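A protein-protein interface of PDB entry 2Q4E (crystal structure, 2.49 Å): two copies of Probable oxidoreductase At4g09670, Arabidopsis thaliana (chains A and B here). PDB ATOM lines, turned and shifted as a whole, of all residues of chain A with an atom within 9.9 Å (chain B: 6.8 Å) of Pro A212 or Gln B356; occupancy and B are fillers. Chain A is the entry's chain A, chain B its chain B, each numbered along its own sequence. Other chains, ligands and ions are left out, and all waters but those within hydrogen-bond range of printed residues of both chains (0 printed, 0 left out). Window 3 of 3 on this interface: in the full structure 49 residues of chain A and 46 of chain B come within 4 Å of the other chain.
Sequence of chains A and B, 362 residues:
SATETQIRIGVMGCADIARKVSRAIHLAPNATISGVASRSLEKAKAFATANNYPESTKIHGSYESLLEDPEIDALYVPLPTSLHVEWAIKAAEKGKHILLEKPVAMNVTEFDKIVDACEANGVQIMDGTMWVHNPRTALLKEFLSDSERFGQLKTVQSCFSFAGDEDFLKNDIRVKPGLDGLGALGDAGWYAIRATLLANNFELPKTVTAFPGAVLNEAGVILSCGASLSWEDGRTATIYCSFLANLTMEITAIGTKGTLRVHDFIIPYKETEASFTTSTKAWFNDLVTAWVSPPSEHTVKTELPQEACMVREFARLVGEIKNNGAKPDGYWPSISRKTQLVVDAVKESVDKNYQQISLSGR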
ATOM      1  N   THR A 209      26.931  19.755   5.568  1.00  0.00           N
ATOM      2  CA  THR A 209      26.850  18.478   6.272  1.00  0.00           C
ATOM      3  C   THR A 209      25.954  17.478   5.544  1.00  0.00           C
ATOM      4  O   THR A 209      24.827  17.797   5.172  1.00  0.00           O
ATOM      5  CB  THR A 209      26.312  18.665   7.705  1.00  0.00           C
ATOM      6  OG1 THR A 209      26.990  19.766   8.333  1.00  0.00           O
ATOM      7  CG2 THR A 209      26.541  17.394   8.529  1.00  0.00           C
ATOM      8  N   ALA A 210      26.460  16.262   5.357  1.00  0.00           N
ATOM      9  CA  ALA A 210      25.717  15.205   4.669  1.00  0.00           C
ATOM     10  C   ALA A 210      24.822  14.421   5.620  1.00  0.00           C
ATOM     11  O   ALA A 210      25.126  14.311   6.804  1.00  0.00           O
ATOM     12  CB  ALA A 210      26.699  14.251   3.979  1.00  0.00           C
ATOM     13  N   PHE A 211      23.719  13.879   5.104  1.00  0.00           N
ATOM     14  CA  PHE A 211      22.819  13.088   5.937  1.00  0.00           C
ATOM     15  C   PHE A 211      23.334  11.663   5.919  1.00  0.00           C
ATOM     16  O   PHE A 211      23.870  11.203   4.912  1.00  0.00           O
ATOM     17  CB  PHE A 211      21.381  13.012   5.391  1.00  0.00           C
ATOM     18  CG  PHE A 211      20.915  14.223   4.642  1.00  0.00           C
ATOM     19  CD1 PHE A 211      21.137  15.503   5.127  1.00  0.00           C
ATOM     20  CD2 PHE A 211      20.169  14.066   3.470  1.00  0.00           C
ATOM     21  CE1 PHE A 211      20.618  16.609   4.463  1.00  0.00           C
ATOM     22  CE2 PHE A 211      19.644  15.168   2.796  1.00  0.00           C
ATOM     23  CZ  PHE A 211      19.869  16.442   3.294  1.00  0.00           C
ATOM     24  N   PRO A 212      23.185  10.944   7.036  1.00  0.00           N
ATOM     25  CA  PRO A 212      23.655   9.558   7.051  1.00  0.00           C
ATOM     26  C   PRO A 212      22.737   8.756   6.120  1.00  0.00           C
ATOM     27  O   PRO A 212      21.716   9.280   5.662  1.00  0.00           O
ATOM     28  CB  PRO A 212      23.491   9.156   8.516  1.00  0.00           C
ATOM     29  CG  PRO A 212      23.695  10.452   9.240  1.00  0.00           C
ATOM     30  CD  PRO A 212      22.893  11.414   8.400  1.00  0.00           C
ATOM     31  N   GLY A 213      23.105   7.508   5.828  1.00  0.00           N
ATOM     32  CA  GLY A 213      22.285   6.676   4.961  1.00  0.00           C
ATOM     33  C   GLY A 213      22.610   6.761   3.483  1.00  0.00           C
ATOM     34  O   GLY A 213      21.743   6.508   2.645  1.00  0.00           O
ATOM     35  N   ALA A 214      23.847   7.127   3.153  1.00  0.00           N
ATOM     36  CA  ALA A 214      24.271   7.219   1.762  1.00  0.00           C
ATOM     37  C   ALA A 214      24.392   5.802   1.201  1.00  0.00           C
ATOM     38  O   ALA A 214      24.558   4.852   1.959  1.00  0.00           O
ATOM     39  CB  ALA A 214      25.607   7.931   1.670  1.00  0.00           C
ATOM     40  N   VAL A 215      24.304   5.661  -0.119  1.00  0.00           N
ATOM     41  CA  VAL A 215      24.408   4.357  -0.762  1.00  0.00           C
ATOM     42  C   VAL A 215      25.508   4.344  -1.823  1.00  0.00           C
ATOM     43  O   VAL A 215      25.439   5.056  -2.824  1.00  0.00           O
ATOM     44  CB  VAL A 215      23.059   3.952  -1.405  1.00  0.00           C
ATOM     45  CG1 VAL A 215      23.185   2.621  -2.147  1.00  0.00           C
ATOM     46  CG2 VAL A 215      22.006   3.848  -0.329  1.00  0.00           C
ATOM     47  N   LEU A 216      26.530   3.536  -1.579  1.00  0.00           N
ATOM     48  CA  LEU A 216      27.656   3.403  -2.494  1.00  0.00           C
ATOM     49  C   LEU A 216      27.707   1.979  -3.042  1.00  0.00           C
ATOM     50  O   LEU A 216      27.433   1.026  -2.306  1.00  0.00           O
ATOM     51  CB  LEU A 216      28.960   3.716  -1.760  1.00  0.00           C
ATOM     52  CG  LEU A 216      29.401   5.176  -1.593  1.00  0.00           C
ATOM     53  CD1 LEU A 216      28.247   6.083  -1.179  1.00  0.00           C
ATOM     54  CD2 LEU A 216      30.506   5.208  -0.554  1.00  0.00           C
ATOM     55  N   SER A 224      23.213   7.333  -3.908  1.00  0.00           N
ATOM     56  CA  SER A 224      22.232   8.224  -3.305  1.00  0.00           C
ATOM     57  C   SER A 224      22.771   8.839  -2.021  1.00  0.00           C
ATOM     58  O   SER A 224      23.429   8.163  -1.222  1.00  0.00           O
ATOM     59  CB  SER A 224      20.907   7.489  -3.030  1.00  0.00           C
ATOM     60  OG  SER A 224      21.026   6.473  -2.048  1.00  0.00           O
ATOM     61  N   CYS A 225      22.506  10.131  -1.840  1.00  0.00           N
ATOM     62  CA  CYS A 225      22.951  10.848  -0.648  1.00  0.00           C
ATOM     63  C   CYS A 225      22.480  12.296  -0.734  1.00  0.00           C
ATOM     64  O   CYS A 225      22.200  12.790  -1.826  1.00  0.00           O
ATOM     65  CB  CYS A 225      24.479  10.814  -0.533  1.00  0.00           C
ATOM     66  SG  CYS A 225      25.355  11.972  -1.629  1.00  0.00           S
ATOM     67  N   GLY A 226      22.390  12.958   0.418  1.00  0.00           N
ATOM     68  CA  GLY A 226      21.970  14.349   0.467  1.00  0.00           C
ATOM     69  C   GLY A 226      22.819  15.142   1.455  1.00  0.00           C
ATOM     70  O   GLY A 226      23.809  14.622   1.983  1.00  0.00           O
ATOM     71  N   ALA A 227      22.446  16.392   1.723  1.00  0.00           N
ATOM     72  CA  ALA A 227      23.219  17.204   2.660  1.00  0.00           C
ATOM     73  C   ALA A 227      22.597  18.564   2.946  1.00  0.00           C
ATOM     74  O   ALA A 227      21.863  19.109   2.126  1.00  0.00           O
ATOM     75  CB  ALA A 227      24.649  17.393   2.133  1.00  0.00           C
ATOM     76  N   SER A 228      22.895  19.109   4.119  1.00  0.00           N
ATOM     77  CA  SER A 228      22.397  20.428   4.502  1.00  0.00           C
ATOM     78  C   SER A 228      23.576  21.398   4.466  1.00  0.00           C
ATOM     79  O   SER A 228      24.676  21.062   4.890  1.00  0.00           O
ATOM     80  CB  SER A 228      21.777  20.383   5.902  1.00  0.00           C
ATOM     81  OG  SER A 228      22.709  19.936   6.864  1.00  0.00           O
ATOM     82  N   TYR A 240      19.616  16.686  -2.741  1.00  0.00           N
ATOM     83  CA  TYR A 240      19.323  15.268  -2.680  1.00  0.00           C
ATOM     84  C   TYR A 240      19.428  14.719  -4.092  1.00  0.00           C
ATOM     85  O   TYR A 240      18.793  15.240  -5.022  1.00  0.00           O
ATOM     86  CB  TYR A 240      17.916  15.025  -2.123  1.00  0.00           C
ATOM     87  CG  TYR A 240      17.648  13.576  -1.782  1.00  0.00           C
ATOM     88  CD1 TYR A 240      18.512  12.881  -0.942  1.00  0.00           C
ATOM     89  CD2 TYR A 240      16.554  12.890  -2.317  1.00  0.00           C
ATOM     90  CE1 TYR A 240      18.308  11.537  -0.640  1.00  0.00           C
ATOM     91  CE2 TYR A 240      16.338  11.539  -2.020  1.00  0.00           C
ATOM     92  CZ  TYR A 240      17.228  10.871  -1.174  1.00  0.00           C
ATOM     93  OH  TYR A 240      17.046   9.542  -0.851  1.00  0.00           O
ATOM     94  N   VAL A 346      30.521  17.890   0.212  1.00  0.00           N
ATOM     95  CA  VAL A 346      29.516  16.847   0.409  1.00  0.00           C
ATOM     96  C   VAL A 346      30.131  15.449   0.345  1.00  0.00           C
ATOM     97  O   VAL A 346      29.751  14.563   1.109  1.00  0.00           O
ATOM     98  CB  VAL A 346      28.400  16.928  -0.645  1.00  0.00           C
ATOM     99  CG1 VAL A 346      27.300  15.953  -0.298  1.00  0.00           C
ATOM    100  CG2 VAL A 346      27.847  18.333  -0.709  1.00  0.00           C
ATOM    101  N   SER A 349      32.433  14.905   3.411  1.00  0.00           N
ATOM    102  CA  SER A 349      31.587  14.641   4.569  1.00  0.00           C
ATOM    103  C   SER A 349      31.083  13.211   4.633  1.00  0.00           C
ATOM    104  O   SER A 349      31.044  12.622   5.709  1.00  0.00           O
ATOM    105  CB  SER A 349      30.390  15.589   4.586  1.00  0.00           C
ATOM    106  OG  SER A 349      29.556  15.311   5.701  1.00  0.00           O
ATOM    107  N   VAL A 350      30.680  12.660   3.490  1.00  0.00           N
ATOM    108  CA  VAL A 350      30.188  11.288   3.450  1.00  0.00           C
ATOM    109  C   VAL A 350      31.220  10.346   4.042  1.00  0.00           C
ATOM    110  O   VAL A 350      30.892   9.506   4.876  1.00  0.00           O
ATOM    111  CB  VAL A 350      29.875  10.824   2.000  1.00  0.00           C
ATOM    112  CG1 VAL A 350      29.702   9.296   1.956  1.00  0.00           C
ATOM    113  CG2 VAL A 350      28.621  11.511   1.498  1.00  0.00           C
ATOM    114  N   ASP A 351      32.469  10.493   3.611  1.00  0.00           N
ATOM    115  CA  ASP A 351      33.553   9.644   4.096  1.00  0.00           C
ATOM    116  C   ASP A 351      34.309  10.170   5.313  1.00  0.00           C
ATOM    117  O   ASP A 351      34.984   9.403   5.997  1.00  0.00           O
ATOM    118  CB  ASP A 351      34.531   9.356   2.958  1.00  0.00           C
ATOM    119  CG  ASP A 351      33.966   8.378   1.955  1.00  0.00           C
ATOM    120  OD1 ASP A 351      33.668   7.239   2.364  1.00  0.00           O
ATOM    121  OD2 ASP A 351      33.812   8.746   0.770  1.00  0.00           O
ATOM    122  N   ASN A 353      33.225  10.893   8.055  1.00  0.00           N
ATOM    123  CA  ASN A 353      32.237  10.669   9.102  1.00  0.00           C
ATOM    124  C   ASN A 353      31.216  11.802   9.256  1.00  0.00           C
ATOM    125  O   ASN A 353      31.149  12.459  10.295  1.00  0.00           O
ATOM    126  CB  ASN A 353      32.955  10.413  10.426  1.00  0.00           C
ATOM    127  CG  ASN A 353      32.159   9.521  11.353  1.00  0.00           C
ATOM    128  OD1 ASN A 353      31.646   8.480  10.938  1.00  0.00           O
ATOM    129  ND2 ASN A 353      32.061   9.916  12.621  1.00  0.00           N
ATOM    130  N   TYR A 354      30.419  12.009   8.215  1.00  0.00           N
ATOM    131  CA  TYR A 354      29.389  13.044   8.189  1.00  0.00           C
ATOM    132  C   TYR A 354      29.695  14.321   8.983  1.00  0.00           C
ATOM    133  O   TYR A 354      28.807  14.899   9.614  1.00  0.00           O
ATOM    134  CB  TYR A 354      28.048  12.445   8.638  1.00  0.00           C
ATOM    135  CG  TYR A 354      27.542  11.406   7.666  1.00  0.00           C
ATOM    136  CD1 TYR A 354      27.257  11.751   6.345  1.00  0.00           C
ATOM    137  CD2 TYR A 354      27.430  10.065   8.036  1.00  0.00           C
ATOM    138  CE1 TYR A 354      26.882  10.791   5.416  1.00  0.00           C
ATOM    139  CE2 TYR A 354      27.054   9.094   7.110  1.00  0.00           C
ATOM    140  CZ  TYR A 354      26.785   9.467   5.800  1.00  0.00           C
ATOM    141  OH  TYR A 354      26.431   8.519   4.867  1.00  0.00           O
ATOM    142  N   GLN A 355      30.953  14.755   8.940  1.00  0.00           N
ATOM    143  CA  GLN A 355      31.381  15.972   9.625  1.00  0.00           C
ATOM    144  C   GLN A 355      30.889  17.176   8.836  1.00  0.00           C
ATOM    145  O   GLN A 355      30.587  17.071   7.639  1.00  0.00           O
ATOM    146  CB  GLN A 355      32.911  16.050   9.703  1.00  0.00           C
ATOM    147  CG  GLN A 355      33.565  15.066  10.643  1.00  0.00           C
ATOM    148  CD  GLN A 355      35.053  14.939  10.396  1.00  0.00           C
ATOM    149  OE1 GLN A 355      35.770  15.930  10.370  1.00  0.00           O
ATOM    150  NE2 GLN A 355      35.524  13.710  10.211  1.00  0.00           N
ATOM    151  N   LYS B 206      15.638   4.255  12.073  1.00  0.00           N
ATOM    152  CA  LYS B 206      16.580   3.562  12.955  1.00  0.00           C
ATOM    153  C   LYS B 206      17.145   4.609  13.894  1.00  0.00           C
ATOM    154  O   LYS B 206      17.181   4.414  15.115  1.00  0.00           O
ATOM    155  CB  LYS B 206      17.733   2.933  12.160  1.00  0.00           C
ATOM    156  CG  LYS B 206      17.421   1.601  11.513  1.00  0.00           C
ATOM    157  CD  LYS B 206      17.265   0.502  12.557  1.00  0.00           C
ATOM    158  CE  LYS B 206      16.924  -0.829  11.907  1.00  0.00           C
ATOM    159  NZ  LYS B 206      16.797  -1.934  12.896  1.00  0.00           N
ATOM    160  N   THR B 207      17.572   5.729  13.307  1.00  0.00           N
ATOM    161  CA  THR B 207      18.155   6.826  14.067  1.00  0.00           C
ATOM    162  C   THR B 207      17.694   8.165  13.522  1.00  0.00           C
ATOM    163  O   THR B 207      17.137   8.240  12.426  1.00  0.00           O
ATOM    164  CB  THR B 207      19.693   6.799  14.001  1.00  0.00           C
ATOM    165  OG1 THR B 207      20.126   7.380  12.764  1.00  0.00           O
ATOM    166  CG2 THR B 207      20.203   5.356  14.083  1.00  0.00           C
ATOM    167  N   VAL B 208      17.940   9.219  14.299  1.00  0.00           N
ATOM    168  CA  VAL B 208      17.566  10.582  13.934  1.00  0.00           C
ATOM    169  C   VAL B 208      18.762  11.513  14.156  1.00  0.00           C
ATOM    170  O   VAL B 208      19.484  11.373  15.138  1.00  0.00           O
ATOM    171  CB  VAL B 208      16.373  11.074  14.800  1.00  0.00           C
ATOM    172  CG1 VAL B 208      16.117  12.561  14.570  1.00  0.00           C
ATOM    173  CG2 VAL B 208      15.133  10.277  14.464  1.00  0.00           C
ATOM    174  N   THR B 209      18.979  12.454  13.243  1.00  0.00           N
ATOM    175  CA  THR B 209      20.096  13.386  13.378  1.00  0.00           C
ATOM    176  C   THR B 209      19.654  14.787  12.970  1.00  0.00           C
ATOM    177  O   THR B 209      19.500  15.074  11.786  1.00  0.00           O
ATOM    178  CB  THR B 209      21.289  12.973  12.483  1.00  0.00           C
ATOM    179  OG1 THR B 209      21.648  11.609  12.742  1.00  0.00           O
ATOM    180  CG2 THR B 209      22.493  13.877  12.765  1.00  0.00           C
ATOM    181  N   ALA B 210      19.447  15.659  13.947  1.00  0.00           N
ATOM    182  CA  ALA B 210      19.020  17.024  13.654  1.00  0.00           C
ATOM    183  C   ALA B 210      20.037  17.728  12.752  1.00  0.00           C
ATOM    184  O   ALA B 210      21.225  17.428  12.818  1.00  0.00           O
ATOM    185  CB  ALA B 210      18.840  17.803  14.954  1.00  0.00           C
ATOM    186  N   PHE B 211      19.571  18.645  11.902  1.00  0.00           N
ATOM    187  CA  PHE B 211      20.465  19.382  11.008  1.00  0.00           C
ATOM    188  C   PHE B 211      21.149  20.538  11.742  1.00  0.00           C
ATOM    189  O   PHE B 211      20.707  20.959  12.811  1.00  0.00           O
ATOM    190  CB  PHE B 211      19.701  19.987   9.823  1.00  0.00           C
ATOM    191  CG  PHE B 211      19.119  18.975   8.867  1.00  0.00           C
ATOM    192  CD1 PHE B 211      19.770  17.774   8.602  1.00  0.00           C
ATOM    193  CD2 PHE B 211      17.941  19.266   8.176  1.00  0.00           C
ATOM    194  CE1 PHE B 211      19.257  16.877   7.660  1.00  0.00           C
ATOM    195  CE2 PHE B 211      17.422  18.383   7.235  1.00  0.00           C
ATOM    196  CZ  PHE B 211      18.082  17.185   6.976  1.00  0.00           C
ATOM    197  N   SER B 228      17.283  14.642   9.172  1.00  0.00           N
ATOM    198  CA  SER B 228      17.061  13.530   8.260  1.00  0.00           C
ATOM    199  C   SER B 228      16.792  12.263   9.058  1.00  0.00           C
ATOM    200  O   SER B 228      17.121  12.194  10.244  1.00  0.00           O
ATOM    201  CB  SER B 228      18.275  13.335   7.338  1.00  0.00           C
ATOM    202  OG  SER B 228      19.486  13.247   8.067  1.00  0.00           O
ATOM    203  N   LEU B 229      16.168  11.278   8.421  1.00  0.00           N
ATOM    204  CA  LEU B 229      15.884  10.012   9.084  1.00  0.00           C
ATOM    205  C   LEU B 229      16.437   8.862   8.238  1.00  0.00           C
ATOM    206  O   LEU B 229      16.518   8.963   7.008  1.00  0.00           O
ATOM    207  CB  LEU B 229      14.375   9.842   9.302  1.00  0.00           C
ATOM    208  CG  LEU B 229      13.680  10.958  10.102  1.00  0.00           C
ATOM    209  CD1 LEU B 229      12.245  10.574  10.404  1.00  0.00           C
ATOM    210  CD2 LEU B 229      14.427  11.206  11.393  1.00  0.00           C
ATOM    211  N   SER B 230      16.838   7.777   8.891  1.00  0.00           N
ATOM    212  CA  SER B 230      17.380   6.648   8.151  1.00  0.00           C
ATOM    213  C   SER B 230      16.866   5.313   8.658  1.00  0.00           C
ATOM    214  O   SER B 230      16.569   5.148   9.841  1.00  0.00           O
ATOM    215  CB  SER B 230      18.912   6.662   8.203  1.00  0.00           C
ATOM    216  OG  SER B 230      19.459   5.673   7.342  1.00  0.00           O
ATOM    217  N   THR B 236      15.243   7.280   3.143  1.00  0.00           N
ATOM    218  CA  THR B 236      15.780   8.423   3.860  1.00  0.00           C
ATOM    219  C   THR B 236      14.818   9.565   3.607  1.00  0.00           C
ATOM    220  O   THR B 236      14.354   9.750   2.483  1.00  0.00           O
ATOM    221  CB  THR B 236      17.177   8.801   3.339  1.00  0.00           C
ATOM    222  OG1 THR B 236      17.148   8.862   1.910  1.00  0.00           O
ATOM    223  CG2 THR B 236      18.212   7.767   3.779  1.00  0.00           C
ATOM    224  N   SER B 349      18.644  15.932  19.572  1.00  0.00           N
ATOM    225  CA  SER B 349      19.897  16.052  18.832  1.00  0.00           C
ATOM    226  C   SER B 349      20.295  17.533  18.699  1.00  0.00           C
ATOM    227  O   SER B 349      21.483  17.865  18.653  1.00  0.00           O
ATOM    228  CB  SER B 349      19.750  15.417  17.442  1.00  0.00           C
ATOM    229  OG  SER B 349      20.953  15.498  16.694  1.00  0.00           O
ATOM    230  N   LYS B 352      22.316  18.197  21.953  1.00  0.00           N
ATOM    231  CA  LYS B 352      23.059  17.005  22.337  1.00  0.00           C
ATOM    232  C   LYS B 352      24.225  16.805  21.363  1.00  0.00           C
ATOM    233  O   LYS B 352      24.634  15.676  21.089  1.00  0.00           O
ATOM    234  CB  LYS B 352      22.124  15.799  22.307  1.00  0.00           C
ATOM    235  CG  LYS B 352      22.026  15.015  23.607  1.00  0.00           C
ATOM    236  CD  LYS B 352      23.190  14.051  23.755  1.00  0.00           C
ATOM    237  CE  LYS B 352      22.924  13.033  24.853  1.00  0.00           C
ATOM    238  NZ  LYS B 352      21.687  12.247  24.579  1.00  0.00           N
ATOM    239  N   ASN B 353      24.734  17.925  20.847  1.00  0.00           N
ATOM    240  CA  ASN B 353      25.852  17.985  19.901  1.00  0.00           C
ATOM    241  C   ASN B 353      25.571  17.357  18.539  1.00  0.00           C
ATOM    242  O   ASN B 353      26.445  16.739  17.932  1.00  0.00           O
ATOM    243  CB  ASN B 353      27.118  17.361  20.508  1.00  0.00           C
ATOM    244  CG  ASN B 353      28.387  17.797  19.782  1.00  0.00           C
ATOM    245  OD1 ASN B 353      28.588  18.986  19.530  1.00  0.00           O
ATOM    246  ND2 ASN B 353      29.250  16.839  19.450  1.00  0.00           N
ATOM    247  N   TYR B 354      24.346  17.531  18.059  1.00  0.00           N
ATOM    248  CA  TYR B 354      23.932  17.004  16.763  1.00  0.00           C
ATOM    249  C   TYR B 354      24.183  15.508  16.664  1.00  0.00           C
ATOM    250  O   TYR B 354      24.651  15.011  15.644  1.00  0.00           O
ATOM    251  CB  TYR B 354      24.668  17.743  15.642  1.00  0.00           C
ATOM    252  CG  TYR B 354      24.519  19.244  15.728  1.00  0.00           C
ATOM    253  CD1 TYR B 354      24.967  19.950  16.853  1.00  0.00           C
ATOM    254  CD2 TYR B 354      23.886  19.954  14.717  1.00  0.00           C
ATOM    255  CE1 TYR B 354      24.774  21.323  16.968  1.00  0.00           C
ATOM    256  CE2 TYR B 354      23.689  21.336  14.821  1.00  0.00           C
ATOM    257  CZ  TYR B 354      24.132  22.009  15.947  1.00  0.00           C
ATOM    258  OH  TYR B 354      23.914  23.361  16.051  1.00  0.00           O
ATOM    259  N   GLN B 355      23.857  14.802  17.745  1.00  0.00           N
ATOM    260  CA  GLN B 355      24.023  13.355  17.826  1.00  0.00           C
ATOM    261  C   GLN B 355      22.963  12.629  17.005  1.00  0.00           C
ATOM    262  O   GLN B 355      21.796  13.032  16.968  1.00  0.00           O
ATOM    263  CB  GLN B 355      23.913  12.894  19.286  1.00  0.00           C
ATOM    264  CG  GLN B 355      24.009  11.373  19.480  1.00  0.00           C
ATOM    265  CD  GLN B 355      23.582  10.916  20.869  1.00  0.00           C
ATOM    266  OE1 GLN B 355      24.036  11.450  21.881  1.00  0.00           O
ATOM    267  NE2 GLN B 355      22.710   9.916  20.919  1.00  0.00           N
ATOM    268  N   GLN B 356      23.367  11.550  16.353  1.00  0.00           N
ATOM    269  CA  GLN B 356      22.433  10.765  15.568  1.00  0.00           C
ATOM    270  C   GLN B 356      21.571   9.907  16.504  1.00  0.00           C
ATOM    271  O   GLN B 356      21.759   8.695  16.613  1.00  0.00           O
ATOM    272  CB  GLN B 356      23.198   9.885  14.571  1.00  0.00           C
ATOM    273  CG  GLN B 356      22.330   8.893  13.807  1.00  0.00           C
ATOM    274  CD  GLN B 356      23.070   8.243  12.658  1.00  0.00           C
ATOM    275  OE1 GLN B 356      24.236   7.876  12.784  1.00  0.00           O
ATOM    276  NE2 GLN B 356      22.389   8.088  11.529  1.00  0.00           N
ATOM    277  N   ILE B 357      20.639  10.554  17.197  1.00  0.00           N
ATOM    278  CA  ILE B 357      19.734   9.873  18.117  1.00  0.00           C
ATOM    279  C   ILE B 357      19.374   8.474  17.634  1.00  0.00           C
ATOM    280  O   ILE B 357      18.869   8.301  16.527  1.00  0.00           O
ATOM    281  CB  ILE B 357      18.430  10.681  18.290  1.00  0.00           C
ATOM    282  CG1 ILE B 357      18.753  12.040  18.905  1.00  0.00           C
ATOM    283  CG2 ILE B 357      17.433   9.904  19.131  1.00  0.00           C
ATOM    284  CD1 ILE B 357      19.627  11.961  20.139  1.00  0.00           C
ATOM    285  N   SER B 358      19.630   7.477  18.474  1.00  0.00           N
ATOM    286  CA  SER B 358      19.335   6.087  18.134  1.00  0.00           C
ATOM    287  C   SER B 358      17.973   5.686  18.686  1.00  0.00           C
ATOM    288  O   SER B 358      17.818   5.478  19.882  1.00  0.00           O
ATOM    289  CB  SER B 358      20.416   5.164  18.706  1.00  0.00           C
ATOM    290  OG  SER B 358      20.078   3.801  18.528  1.00  0.00           O
ATOM    291  N   LEU B 359      16.983   5.576  17.810  1.00  0.00           N
ATOM    292  CA  LEU B 359      15.650   5.203  18.247  1.00  0.00           C
ATOM    293  C   LEU B 359      15.529   3.695  18.423  1.00  0.00           C
ATOM    294  O   LEU B 359      14.868   3.015  17.637  1.00  0.00           O
ATOM    295  CB  LEU B 359      14.606   5.720  17.252  1.00  0.00           C
ATOM    296  CG  LEU B 359      14.555   7.250  17.129  1.00  0.00           C
ATOM    297  CD1 LEU B 359      13.428   7.658  16.192  1.00  0.00           C
ATOM    298  CD2 LEU B 359      14.344   7.877  18.504  1.00  0.00           C
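Among the printed residues, merely in contact across the chains: Phe A211 with Ser B228 (3.3 Å), Pro A212 with Gln B356 (3.4 Å), Phe A211 with Phe B211 (3.4 Å), Gly A213 with Ser B230 (3.8 Å), Pro A212 with Ser B228 (3.9 Å) and Gly A213 with Thr B236 (3.9 Å).
The backbone NH (N) of Ser B228 sits at hydrogen-bond distance from the backbone carbonyl oxygen (O) of Thr B209.
N of Phe A211 sits at hydrogen-bond distance from O of Gly A226 (3.2 Å).
OG1 of Thr B207 lies within hydrogen-bond range of NE2 of Gln B356 (2.7 Å).
The backbone carbonyl oxygen (O) of Ser B230 is in hydrogen-bond range of the backbone NH (N) of Lys B206 (2.6 Å).
Pro A212 touches just these residues of chain B: Ser B228 and Gln B356.
Of the printed residues of chain B, Tyr A240 touches Thr B236 (2.8 Å).
Val A350 touches none of the printed residues of chain B.
Thr B207 touches none of the printed residues of chain A.
Printed residues of chain A within 4 Å of Phe B211: Phe A211.
Printed residues of chain A within 4 Å of Ser B230: Gly A213.
Asn B353 touches none of the printed residues of chain A.
No residue of chain A comes within 4 Å of Gln B355.
Gln B356 touches just one residue of chain A: Pro A212 (3.4 Å).
The nearest residue of chain B that does not touch Pro A212 is Thr B209 (4.2 Å).
The nearest residue of chain A that does not touch Gln B356 is Gly A213 (5.8 Å).
OG1 of Thr B236 is in hydrogen-bond range of OH of Tyr A240, 2.8 Å away.
Printed residues of chain B that touch a printed residue of chain A: Phe B211, Ser B228, Ser B230, Thr B236 and Gln B356.
Hydrophobic or aromatic side chains of chain B that line the printed part of chain A: Phe B211.
Along chain B the printed residues that touch a printed residue of chain A span positions 211 to 356.
Of the 21 printed residues of chain A, 4 touch a printed residue of chain B.
Hydrophobic or aromatic side chains of chain A within 4 Å of the printed part of chain B: Phe A211, Pro A212 and Tyr A240.
Among the printed residues, 7 pairs touch across the chains.
Among the printed residues, no Asp or Glu carboxylate lies within 4 Å of a Lys or Arg side-chain nitrogen of the other chain.
Phe B211 touches its own counterpart, Phe A211.
Phe A211 touches Ser B228, but with the chains exchanged Ser A228 does not touch Phe B211 (4.04 Å).
Of the 7 pairs that touch across the chains among the printed residues, 1 has its exchanged pair printed and touching as well.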
